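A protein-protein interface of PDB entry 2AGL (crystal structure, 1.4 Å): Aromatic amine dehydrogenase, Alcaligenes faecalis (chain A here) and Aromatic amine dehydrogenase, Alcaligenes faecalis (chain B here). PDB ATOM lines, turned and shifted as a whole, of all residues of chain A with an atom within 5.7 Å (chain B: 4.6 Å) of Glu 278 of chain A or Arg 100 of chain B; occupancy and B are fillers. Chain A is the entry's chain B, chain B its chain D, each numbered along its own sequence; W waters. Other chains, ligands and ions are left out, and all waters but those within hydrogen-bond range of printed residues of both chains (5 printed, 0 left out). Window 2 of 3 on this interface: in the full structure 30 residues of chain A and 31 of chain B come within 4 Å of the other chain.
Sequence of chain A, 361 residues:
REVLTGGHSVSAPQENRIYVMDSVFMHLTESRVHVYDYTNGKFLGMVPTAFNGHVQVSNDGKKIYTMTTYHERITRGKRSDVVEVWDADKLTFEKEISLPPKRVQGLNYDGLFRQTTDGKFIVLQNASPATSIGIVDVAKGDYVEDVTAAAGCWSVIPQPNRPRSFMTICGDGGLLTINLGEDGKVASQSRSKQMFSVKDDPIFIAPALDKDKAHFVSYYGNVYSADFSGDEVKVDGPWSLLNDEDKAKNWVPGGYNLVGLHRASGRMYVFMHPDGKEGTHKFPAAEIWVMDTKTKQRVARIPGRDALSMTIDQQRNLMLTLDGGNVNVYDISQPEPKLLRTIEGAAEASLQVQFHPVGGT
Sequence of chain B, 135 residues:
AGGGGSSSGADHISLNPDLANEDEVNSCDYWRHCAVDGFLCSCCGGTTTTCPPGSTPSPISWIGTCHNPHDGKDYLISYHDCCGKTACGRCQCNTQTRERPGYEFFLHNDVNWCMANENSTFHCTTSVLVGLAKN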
ATOM      1  N   VAL A 198     -16.189   8.909   1.530  1.00  0.00           N
ATOM      2  CA  VAL A 198     -16.987   8.143   2.470  1.00  0.00           C
ATOM      3  C   VAL A 198     -17.725   9.058   3.439  1.00  0.00           C
ATOM      4  O   VAL A 198     -18.897   8.842   3.738  1.00  0.00           O
ATOM      5  CB  VAL A 198     -16.114   7.085   3.190  1.00  0.00           C
ATOM      6  CG1 VAL A 198     -16.854   6.457   4.333  1.00  0.00           C
ATOM      7  CG2 VAL A 198     -15.720   6.016   2.197  1.00  0.00           C
ATOM      8  N   LYS A 199     -17.066  10.103   3.924  1.00  0.00           N
ATOM      9  CA  LYS A 199     -17.686  10.999   4.893  1.00  0.00           C
ATOM     10  C   LYS A 199     -18.705  11.959   4.259  1.00  0.00           C
ATOM     11  O   LYS A 199     -19.774  12.197   4.816  1.00  0.00           O
ATOM     12  CB  LYS A 199     -16.598  11.805   5.634  1.00  0.00           C
ATOM     13  N   PRO A 202     -21.433   9.450   0.795  1.00  0.00           N
ATOM     14  CA  PRO A 202     -21.468   7.988   0.779  1.00  0.00           C
ATOM     15  C   PRO A 202     -22.361   7.451  -0.332  1.00  0.00           C
ATOM     16  O   PRO A 202     -23.446   8.011  -0.575  1.00  0.00           O
ATOM     17  CB  PRO A 202     -22.066   7.642   2.139  1.00  0.00           C
ATOM     18  CG  PRO A 202     -22.774   8.839   2.602  1.00  0.00           C
ATOM     19  CD  PRO A 202     -21.966   9.990   2.055  1.00  0.00           C
ATOM     20  N   TYR A 219     -26.032   9.062  -1.301  1.00  0.00           N
ATOM     21  CA  TYR A 219     -27.057   9.530  -0.368  1.00  0.00           C
ATOM     22  C   TYR A 219     -27.630  10.909  -0.722  1.00  0.00           C
ATOM     23  O   TYR A 219     -28.752  11.233  -0.313  1.00  0.00           O
ATOM     24  CB  TYR A 219     -26.515   9.594   1.046  1.00  0.00           C
ATOM     25  CG  TYR A 219     -26.448   8.289   1.843  1.00  0.00           C
ATOM     26  CD1 TYR A 219     -26.695   8.314   3.197  1.00  0.00           C
ATOM     27  CD2 TYR A 219     -26.091   7.074   1.260  1.00  0.00           C
ATOM     28  CE1 TYR A 219     -26.612   7.172   3.965  1.00  0.00           C
ATOM     29  CE2 TYR A 219     -26.015   5.902   2.053  1.00  0.00           C
ATOM     30  CZ  TYR A 219     -26.283   5.998   3.389  1.00  0.00           C
ATOM     31  OH  TYR A 219     -26.183   4.898   4.229  1.00  0.00           O
ATOM     32  N   TYR A 220     -26.843  11.731  -1.431  1.00  0.00           N
ATOM     33  CA  TYR A 220     -27.243  13.096  -1.791  1.00  0.00           C
ATOM     34  C   TYR A 220     -27.607  13.220  -3.264  1.00  0.00           C
ATOM     35  O   TYR A 220     -27.790  14.337  -3.776  1.00  0.00           O
ATOM     36  CB  TYR A 220     -26.116  14.066  -1.385  1.00  0.00           C
ATOM     37  CG  TYR A 220     -25.789  13.985   0.094  1.00  0.00           C
ATOM     38  CD1 TYR A 220     -24.571  13.475   0.534  1.00  0.00           C
ATOM     39  CD2 TYR A 220     -26.695  14.402   1.063  1.00  0.00           C
ATOM     40  CE1 TYR A 220     -24.268  13.391   1.886  1.00  0.00           C
ATOM     41  CE2 TYR A 220     -26.405  14.313   2.430  1.00  0.00           C
ATOM     42  CZ  TYR A 220     -25.182  13.802   2.833  1.00  0.00           C
ATOM     43  OH  TYR A 220     -24.881  13.708   4.171  1.00  0.00           O
ATOM     44  N   GLY A 276     -35.545  14.868   1.321  1.00  0.00           N
ATOM     45  CA  GLY A 276     -34.380  14.133   1.793  1.00  0.00           C
ATOM     46  C   GLY A 276     -33.697  14.809   2.958  1.00  0.00           C
ATOM     47  O   GLY A 276     -33.648  16.032   3.047  1.00  0.00           O
ATOM     48  N   LYS A 277     -33.202  14.006   3.882  1.00  0.00           N
ATOM     49  CA  LYS A 277     -32.379  14.504   4.966  1.00  0.00           C
ATOM     50  C   LYS A 277     -31.693  13.301   5.588  1.00  0.00           C
ATOM     51  O   LYS A 277     -31.924  12.166   5.155  1.00  0.00           O
ATOM     52  CB  LYS A 277     -33.201  15.261   5.998  1.00  0.00           C
ATOM     53  CG  LYS A 277     -34.259  14.429   6.713  1.00  0.00           C
ATOM     54  CD  LYS A 277     -35.201  15.271   7.540  1.00  0.00           C
ATOM     55  CE  LYS A 277     -35.960  16.284   6.695  1.00  0.00           C
ATOM     56  NZ  LYS A 277     -37.049  16.953   7.469  1.00  0.00           N
ATOM     57  N   GLU A 278     -30.857  13.557   6.582  1.00  0.00           N
ATOM     58  CA  GLU A 278     -30.164  12.488   7.253  1.00  0.00           C
ATOM     59  C   GLU A 278     -31.186  11.484   7.757  1.00  0.00           C
ATOM     60  O   GLU A 278     -32.104  11.838   8.501  1.00  0.00           O
ATOM     61  CB  GLU A 278     -29.340  13.035   8.416  1.00  0.00           C
ATOM     62  CG  GLU A 278     -28.557  11.967   9.175  1.00  0.00           C
ATOM     63  CD  GLU A 278     -27.582  11.221   8.288  1.00  0.00           C
ATOM     64  OE1 GLU A 278     -26.643  11.849   7.727  1.00  0.00           O
ATOM     65  OE2 GLU A 278     -27.732   9.973   8.144  1.00  0.00           O
ATOM     66  N   GLY A 279     -31.026  10.226   7.340  1.00  0.00           N
ATOM     67  CA  GLY A 279     -31.870   9.145   7.835  1.00  0.00           C
ATOM     68  C   GLY A 279     -32.946   8.660   6.884  1.00  0.00           C
ATOM     69  O   GLY A 279     -33.695   7.759   7.265  1.00  0.00           O
ATOM     70  N   THR A 280     -33.030   9.210   5.678  1.00  0.00           N
ATOM     71  CA  THR A 280     -34.085   8.821   4.725  1.00  0.00           C
ATOM     72  C   THR A 280     -33.583   7.948   3.583  1.00  0.00           C
ATOM     73  O   THR A 280     -34.282   7.736   2.617  1.00  0.00           O
ATOM     74  CB  THR A 280     -34.841  10.081   4.153  1.00  0.00           C
ATOM     75  OG1 THR A 280     -34.052  10.762   3.157  1.00  0.00           O
ATOM     76  CG2 THR A 280     -35.155  11.067   5.232  1.00  0.00           C
ATOM     77  N   HIS A 281     -32.367   7.399   3.664  1.00  0.00           N
ATOM     78  CA  HIS A 281     -31.770   6.685   2.554  1.00  0.00           C
ATOM     79  C   HIS A 281     -32.385   5.302   2.222  1.00  0.00           C
ATOM     80  O   HIS A 281     -32.097   4.730   1.172  1.00  0.00           O
ATOM     81  CB  HIS A 281     -30.234   6.558   2.716  1.00  0.00           C
ATOM     82  CG  HIS A 281     -29.776   6.041   4.047  1.00  0.00           C
ATOM     83  ND1 HIS A 281     -29.732   6.823   5.175  1.00  0.00           N
ATOM     84  CD2 HIS A 281     -29.295   4.822   4.416  1.00  0.00           C
ATOM     85  CE1 HIS A 281     -29.272   6.110   6.189  1.00  0.00           C
ATOM     86  NE2 HIS A 281     -28.985   4.899   5.744  1.00  0.00           N
ATOM     87  N   GLN B  96     -32.668   5.126  10.741  1.00  0.00           N
ATOM     88  CA  GLN B  96     -31.447   5.108   9.968  1.00  0.00           C
ATOM     89  C   GLN B  96     -30.607   6.382  10.112  1.00  0.00           C
ATOM     90  O   GLN B  96     -29.806   6.671   9.238  1.00  0.00           O
ATOM     91  CB  GLN B  96     -31.801   4.897   8.495  1.00  0.00           C
ATOM     92  CG  GLN B  96     -32.569   3.577   8.184  1.00  0.00           C
ATOM     93  CD  GLN B  96     -31.684   2.375   8.395  1.00  0.00           C
ATOM     94  OE1 GLN B  96     -32.154   1.250   8.735  1.00  0.00           O
ATOM     95  NE2 GLN B  96     -30.422   2.566   8.150  1.00  0.00           N
ATOM     96  N   THR B  97     -30.820   7.110  11.196  1.00  0.00           N
ATOM     97  CA  THR B  97     -30.045   8.343  11.453  1.00  0.00           C
ATOM     98  C   THR B  97     -28.556   8.013  11.499  1.00  0.00           C
ATOM     99  O   THR B  97     -28.127   7.244  12.346  1.00  0.00           O
ATOM    100  CB  THR B  97     -30.479   8.968  12.755  1.00  0.00           C
ATOM    101  OG1 THR B  97     -31.832   9.446  12.635  1.00  0.00           O
ATOM    102  CG2 THR B  97     -29.649  10.246  13.070  1.00  0.00           C
ATOM    103  N   ARG B  98     -27.800   8.608  10.577  1.00  0.00           N
ATOM    104  CA  ARG B  98     -26.333   8.487  10.471  1.00  0.00           C
ATOM    105  C   ARG B  98     -25.831   7.073  10.172  1.00  0.00           C
ATOM    106  O   ARG B  98     -24.638   6.817  10.185  1.00  0.00           O
ATOM    107  CB  ARG B  98     -25.644   9.141  11.663  1.00  0.00           C
ATOM    108  CG  ARG B  98     -25.662  10.682  11.548  1.00  0.00           C
ATOM    109  CD  ARG B  98     -25.048  11.455  12.696  1.00  0.00           C
ATOM    110  NE  ARG B  98     -25.949  11.588  13.831  1.00  0.00           N
ATOM    111  CZ  ARG B  98     -27.030  12.381  13.873  1.00  0.00           C
ATOM    112  NH1 ARG B  98     -27.368  13.146  12.835  1.00  0.00           N
ATOM    113  NH2 ARG B  98     -27.781  12.409  14.981  1.00  0.00           N
ATOM    114  N   GLU B  99     -26.752   6.200   9.763  1.00  0.00           N
ATOM    115  CA  GLU B  99     -26.409   4.836   9.382  1.00  0.00           C
ATOM    116  C   GLU B  99     -25.749   4.838   8.018  1.00  0.00           C
ATOM    117  O   GLU B  99     -26.104   5.611   7.118  1.00  0.00           O
ATOM    118  CB  GLU B  99     -27.681   3.958   9.342  1.00  0.00           C
ATOM    119  CG  GLU B  99     -27.424   2.450   9.208  1.00  0.00           C
ATOM    120  CD  GLU B  99     -27.303   1.933   7.788  1.00  0.00           C
ATOM    121  OE1 GLU B  99     -27.492   2.688   6.793  1.00  0.00           O
ATOM    122  OE2 GLU B  99     -27.050   0.724   7.603  1.00  0.00           O
ATOM    123  N   ARG B 100     -24.752   3.997   7.843  1.00  0.00           N
ATOM    124  CA  ARG B 100     -24.015   3.904   6.619  1.00  0.00           C
ATOM    125  C   ARG B 100     -23.828   2.455   6.131  1.00  0.00           C
ATOM    126  O   ARG B 100     -24.050   1.522   6.904  1.00  0.00           O
ATOM    127  CB  ARG B 100     -22.659   4.601   6.813  1.00  0.00           C
ATOM    128  CG  ARG B 100     -22.758   6.122   7.120  1.00  0.00           C
ATOM    129  CD  ARG B 100     -23.250   6.902   5.920  1.00  0.00           C
ATOM    130  NE  ARG B 100     -23.317   8.348   6.134  1.00  0.00           N
ATOM    131  CZ  ARG B 100     -24.365   9.013   6.606  1.00  0.00           C
ATOM    132  NH1 ARG B 100     -25.480   8.393   6.968  1.00  0.00           N
ATOM    133  NH2 ARG B 100     -24.300  10.335   6.702  1.00  0.00           N
ATOM    134  N   PRO B 101     -23.501   2.255   4.860  1.00  0.00           N
ATOM    135  CA  PRO B 101     -23.387   0.891   4.294  1.00  0.00           C
ATOM    136  C   PRO B 101     -22.234   0.067   4.862  1.00  0.00           C
ATOM    137  O   PRO B 101     -21.457   0.576   5.671  1.00  0.00           O
ATOM    138  CB  PRO B 101     -23.214   1.137   2.798  1.00  0.00           C
ATOM    139  CG  PRO B 101     -23.753   2.557   2.617  1.00  0.00           C
ATOM    140  CD  PRO B 101     -23.247   3.272   3.814  1.00  0.00           C
ATOM    141  N   GLY B 102     -22.127  -1.186   4.430  1.00  0.00           N
ATOM    142  CA  GLY B 102     -21.222  -2.160   5.050  1.00  0.00           C
ATOM    143  C   GLY B 102     -19.743  -1.848   4.877  1.00  0.00           C
ATOM    144  O   GLY B 102     -18.933  -2.442   5.580  1.00  0.00           O
ATOM    145  N   GLU B 104     -18.595   0.892   5.860  1.00  0.00           N
ATOM    146  CA  GLU B 104     -18.349   1.496   7.180  1.00  0.00           C
ATOM    147  C   GLU B 104     -19.070   0.601   8.204  1.00  0.00           C
ATOM    148  O   GLU B 104     -20.120   0.947   8.762  1.00  0.00           O
ATOM    149  CB  GLU B 104     -18.874   2.944   7.267  1.00  0.00           C
ATOM    150  CG  GLU B 104     -18.456   3.907   6.157  1.00  0.00           C
ATOM    151  CD  GLU B 104     -19.126   5.279   6.287  1.00  0.00           C
ATOM    152  OE1 GLU B 104     -18.958   5.933   7.330  1.00  0.00           O
ATOM    153  OE2 GLU B 104     -19.826   5.719   5.333  1.00  0.00           O
ATOM    154  N   LEU B 107     -21.102   1.165  11.531  1.00  0.00           N
ATOM    155  CA  LEU B 107     -22.206   2.119  11.451  1.00  0.00           C
ATOM    156  C   LEU B 107     -23.392   1.515  10.708  1.00  0.00           C
ATOM    157  O   LEU B 107     -24.354   2.215  10.453  1.00  0.00           O
ATOM    158  CB  LEU B 107     -21.753   3.384  10.696  1.00  0.00           C
ATOM    159  CG  LEU B 107     -20.666   4.215  11.359  1.00  0.00           C
ATOM    160  CD1 LEU B 107     -20.349   5.432  10.472  1.00  0.00           C
ATOM    161  CD2 LEU B 107     -21.061   4.675  12.712  1.00  0.00           C
ATOM    162  N   HIS B 108     -23.324   0.228  10.355  1.00  0.00           N
ATOM    163  CA  HIS B 108     -24.242  -0.387   9.419  1.00  0.00           C
ATOM    164  C   HIS B 108     -25.260  -1.277  10.141  1.00  0.00           C
ATOM    165  O   HIS B 108     -24.883  -2.152  10.942  1.00  0.00           O
ATOM    166  CB  HIS B 108     -23.447  -1.258   8.448  1.00  0.00           C
ATOM    167  CG  HIS B 108     -24.285  -1.824   7.353  1.00  0.00           C
ATOM    168  ND1 HIS B 108     -24.204  -3.126   6.910  1.00  0.00           N
ATOM    169  CD2 HIS B 108     -25.240  -1.232   6.606  1.00  0.00           C
ATOM    170  CE1 HIS B 108     -25.084  -3.312   5.939  1.00  0.00           C
ATOM    171  NE2 HIS B 108     -25.713  -2.173   5.730  1.00  0.00           N
HETATM  172  O   HOH W   1     -22.558  12.078   5.135  1.00  0.00           O
HETATM  173  O   HOH W   2     -24.643  13.127   8.629  1.00  0.00           O
HETATM  174  O   HOH W   3     -20.380   8.200   5.634  1.00  0.00           O
HETATM  175  O   HOH W   4     -26.710   1.701   4.401  1.00  0.00           O
HETATM  176  O   HOH W   5     -34.743   6.989   9.675  1.00  0.00           O
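The guanidinium group (NH2) of Arg 100 of chain B lies within salt-bridge range of the side-chain carboxylate (OE1) of Glu 278 of chain A (3.0 Å).
The side-chain carboxylate of Glu 278 of chain A lies within hydrogen-bond range of the backbone NH of Arg 98 of chain B, at 2.8 Å.
The backbone carbonyl oxygen (O) of Glu 99 of chain B sits at hydrogen-bond distance from the side-chain hydroxyl (OH) of Tyr 219 of chain A, 3.0 Å away.
A ring nitrogen (NE2) of His 281 of chain A sits at hydrogen-bond distance from the side-chain carboxylate (OE1) of Glu 99 of chain B.
OH of Tyr 219 of chain A lies close to NE2 of His 281 of chain A (3.2 Å).
The side-chain amide nitrogen of Gln 96 of chain B lies close to the side-chain carboxylate of Glu 99 of chain B (3.2 Å).
N of Tyr 219 of chain A sits at hydrogen-bond distance from O of Pro 202 of chain A, at 2.9 Å.
N of Arg 100 of chain B sits at hydrogen-bond distance from O of Leu 107 of chain B (3.2 Å).
Among the printed residues, pairs that only touch across the chains: His 281 of chain A with Gln 96 of chain B (3.1 Å), Val 198 of chain A with Glu 104 of chain B (3.2 Å), Tyr 219 of chain A with Arg 100 of chain B (3.4 Å), Tyr 219 of chain A with Pro 101 of chain B (3.4 Å), Gly 279 of chain A with Gln 96 of chain B (3.5 Å), Pro 202 of chain A with Arg 100 of chain B (3.6 Å) and Glu 278 of chain A with Thr 97 of chain B (3.97 Å).
Of the 11 printed residues of chain A, 6 touch a printed residue of chain B.
Of the 10 printed residues of chain B, 7 touch a printed residue of chain A.
Hydrophobic or aromatic side chains of chain B that line the printed part of chain A: Pro 101.
Among the printed residues, 11 pairs touch across the chains.
Among the printed residues, Asp or Glu carboxylates within 4 Å of a Lys or Arg side-chain nitrogen of the other chain: Glu 278 of chain A with Arg 100 of chain B (3.0 Å).
Printed residues of chain B within 4 Å of Val 198 of chain A: Glu 104.
Lys 199 of chain A touches none of the printed residues of chain B.
Of the printed residues of chain B, Tyr 219 of chain A touches Glu 99, Arg 100 and Pro 101.
Glu 278 of chain A touches just these residues of chain B: Thr 97 (3.97 Å), Arg 98 (2.8 Å) and Arg 100 (3.0 Å).
Printed residues of chain B within 4 Å of His 281 of chain A: Gln 96 and Glu 99.
Of chain A, only Pro 202, Tyr 219 and Glu 278 come within 4 Å of Arg 100 of chain B.
His 108 of chain B touches none of the printed residues of chain A.
The nearest residue of chain B that does not touch Glu 278 of chain A is Gln 96 of chain B (4.05 Å).
Water W3 lies within hydrogen-bond range of the backbone carbonyl oxygen (O) of Val 198 of chain A (2.5 Å), the side-chain carboxylate (OE2) of Glu 104 of chain B (2.6 Å) and the guanidinium group (NE) of Arg 100 of chain B (3.0 Å).
Water W2 bridges OE1 of Glu 278 of chain A (2.5 Å) and NH2 of Arg 100 of chain B (3.4 Å).
Water W4 lies within hydrogen-bond range of OE1 of Glu 99 of chain B and OH of Tyr 219 of chain A.
Water W5 lies within hydrogen-bond range of the backbone carbonyl oxygen of Gly 279 of chain A (2.7 Å) and the backbone NH of Gln 96 of chain B (3.0 Å).
Water W1 lies within hydrogen-bond range of the backbone carbonyl oxygen of Lys 199 of chain A, the guanidinium group of Arg 100 of chain B and the side-chain hydroxyl of Tyr 220 of chain A.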
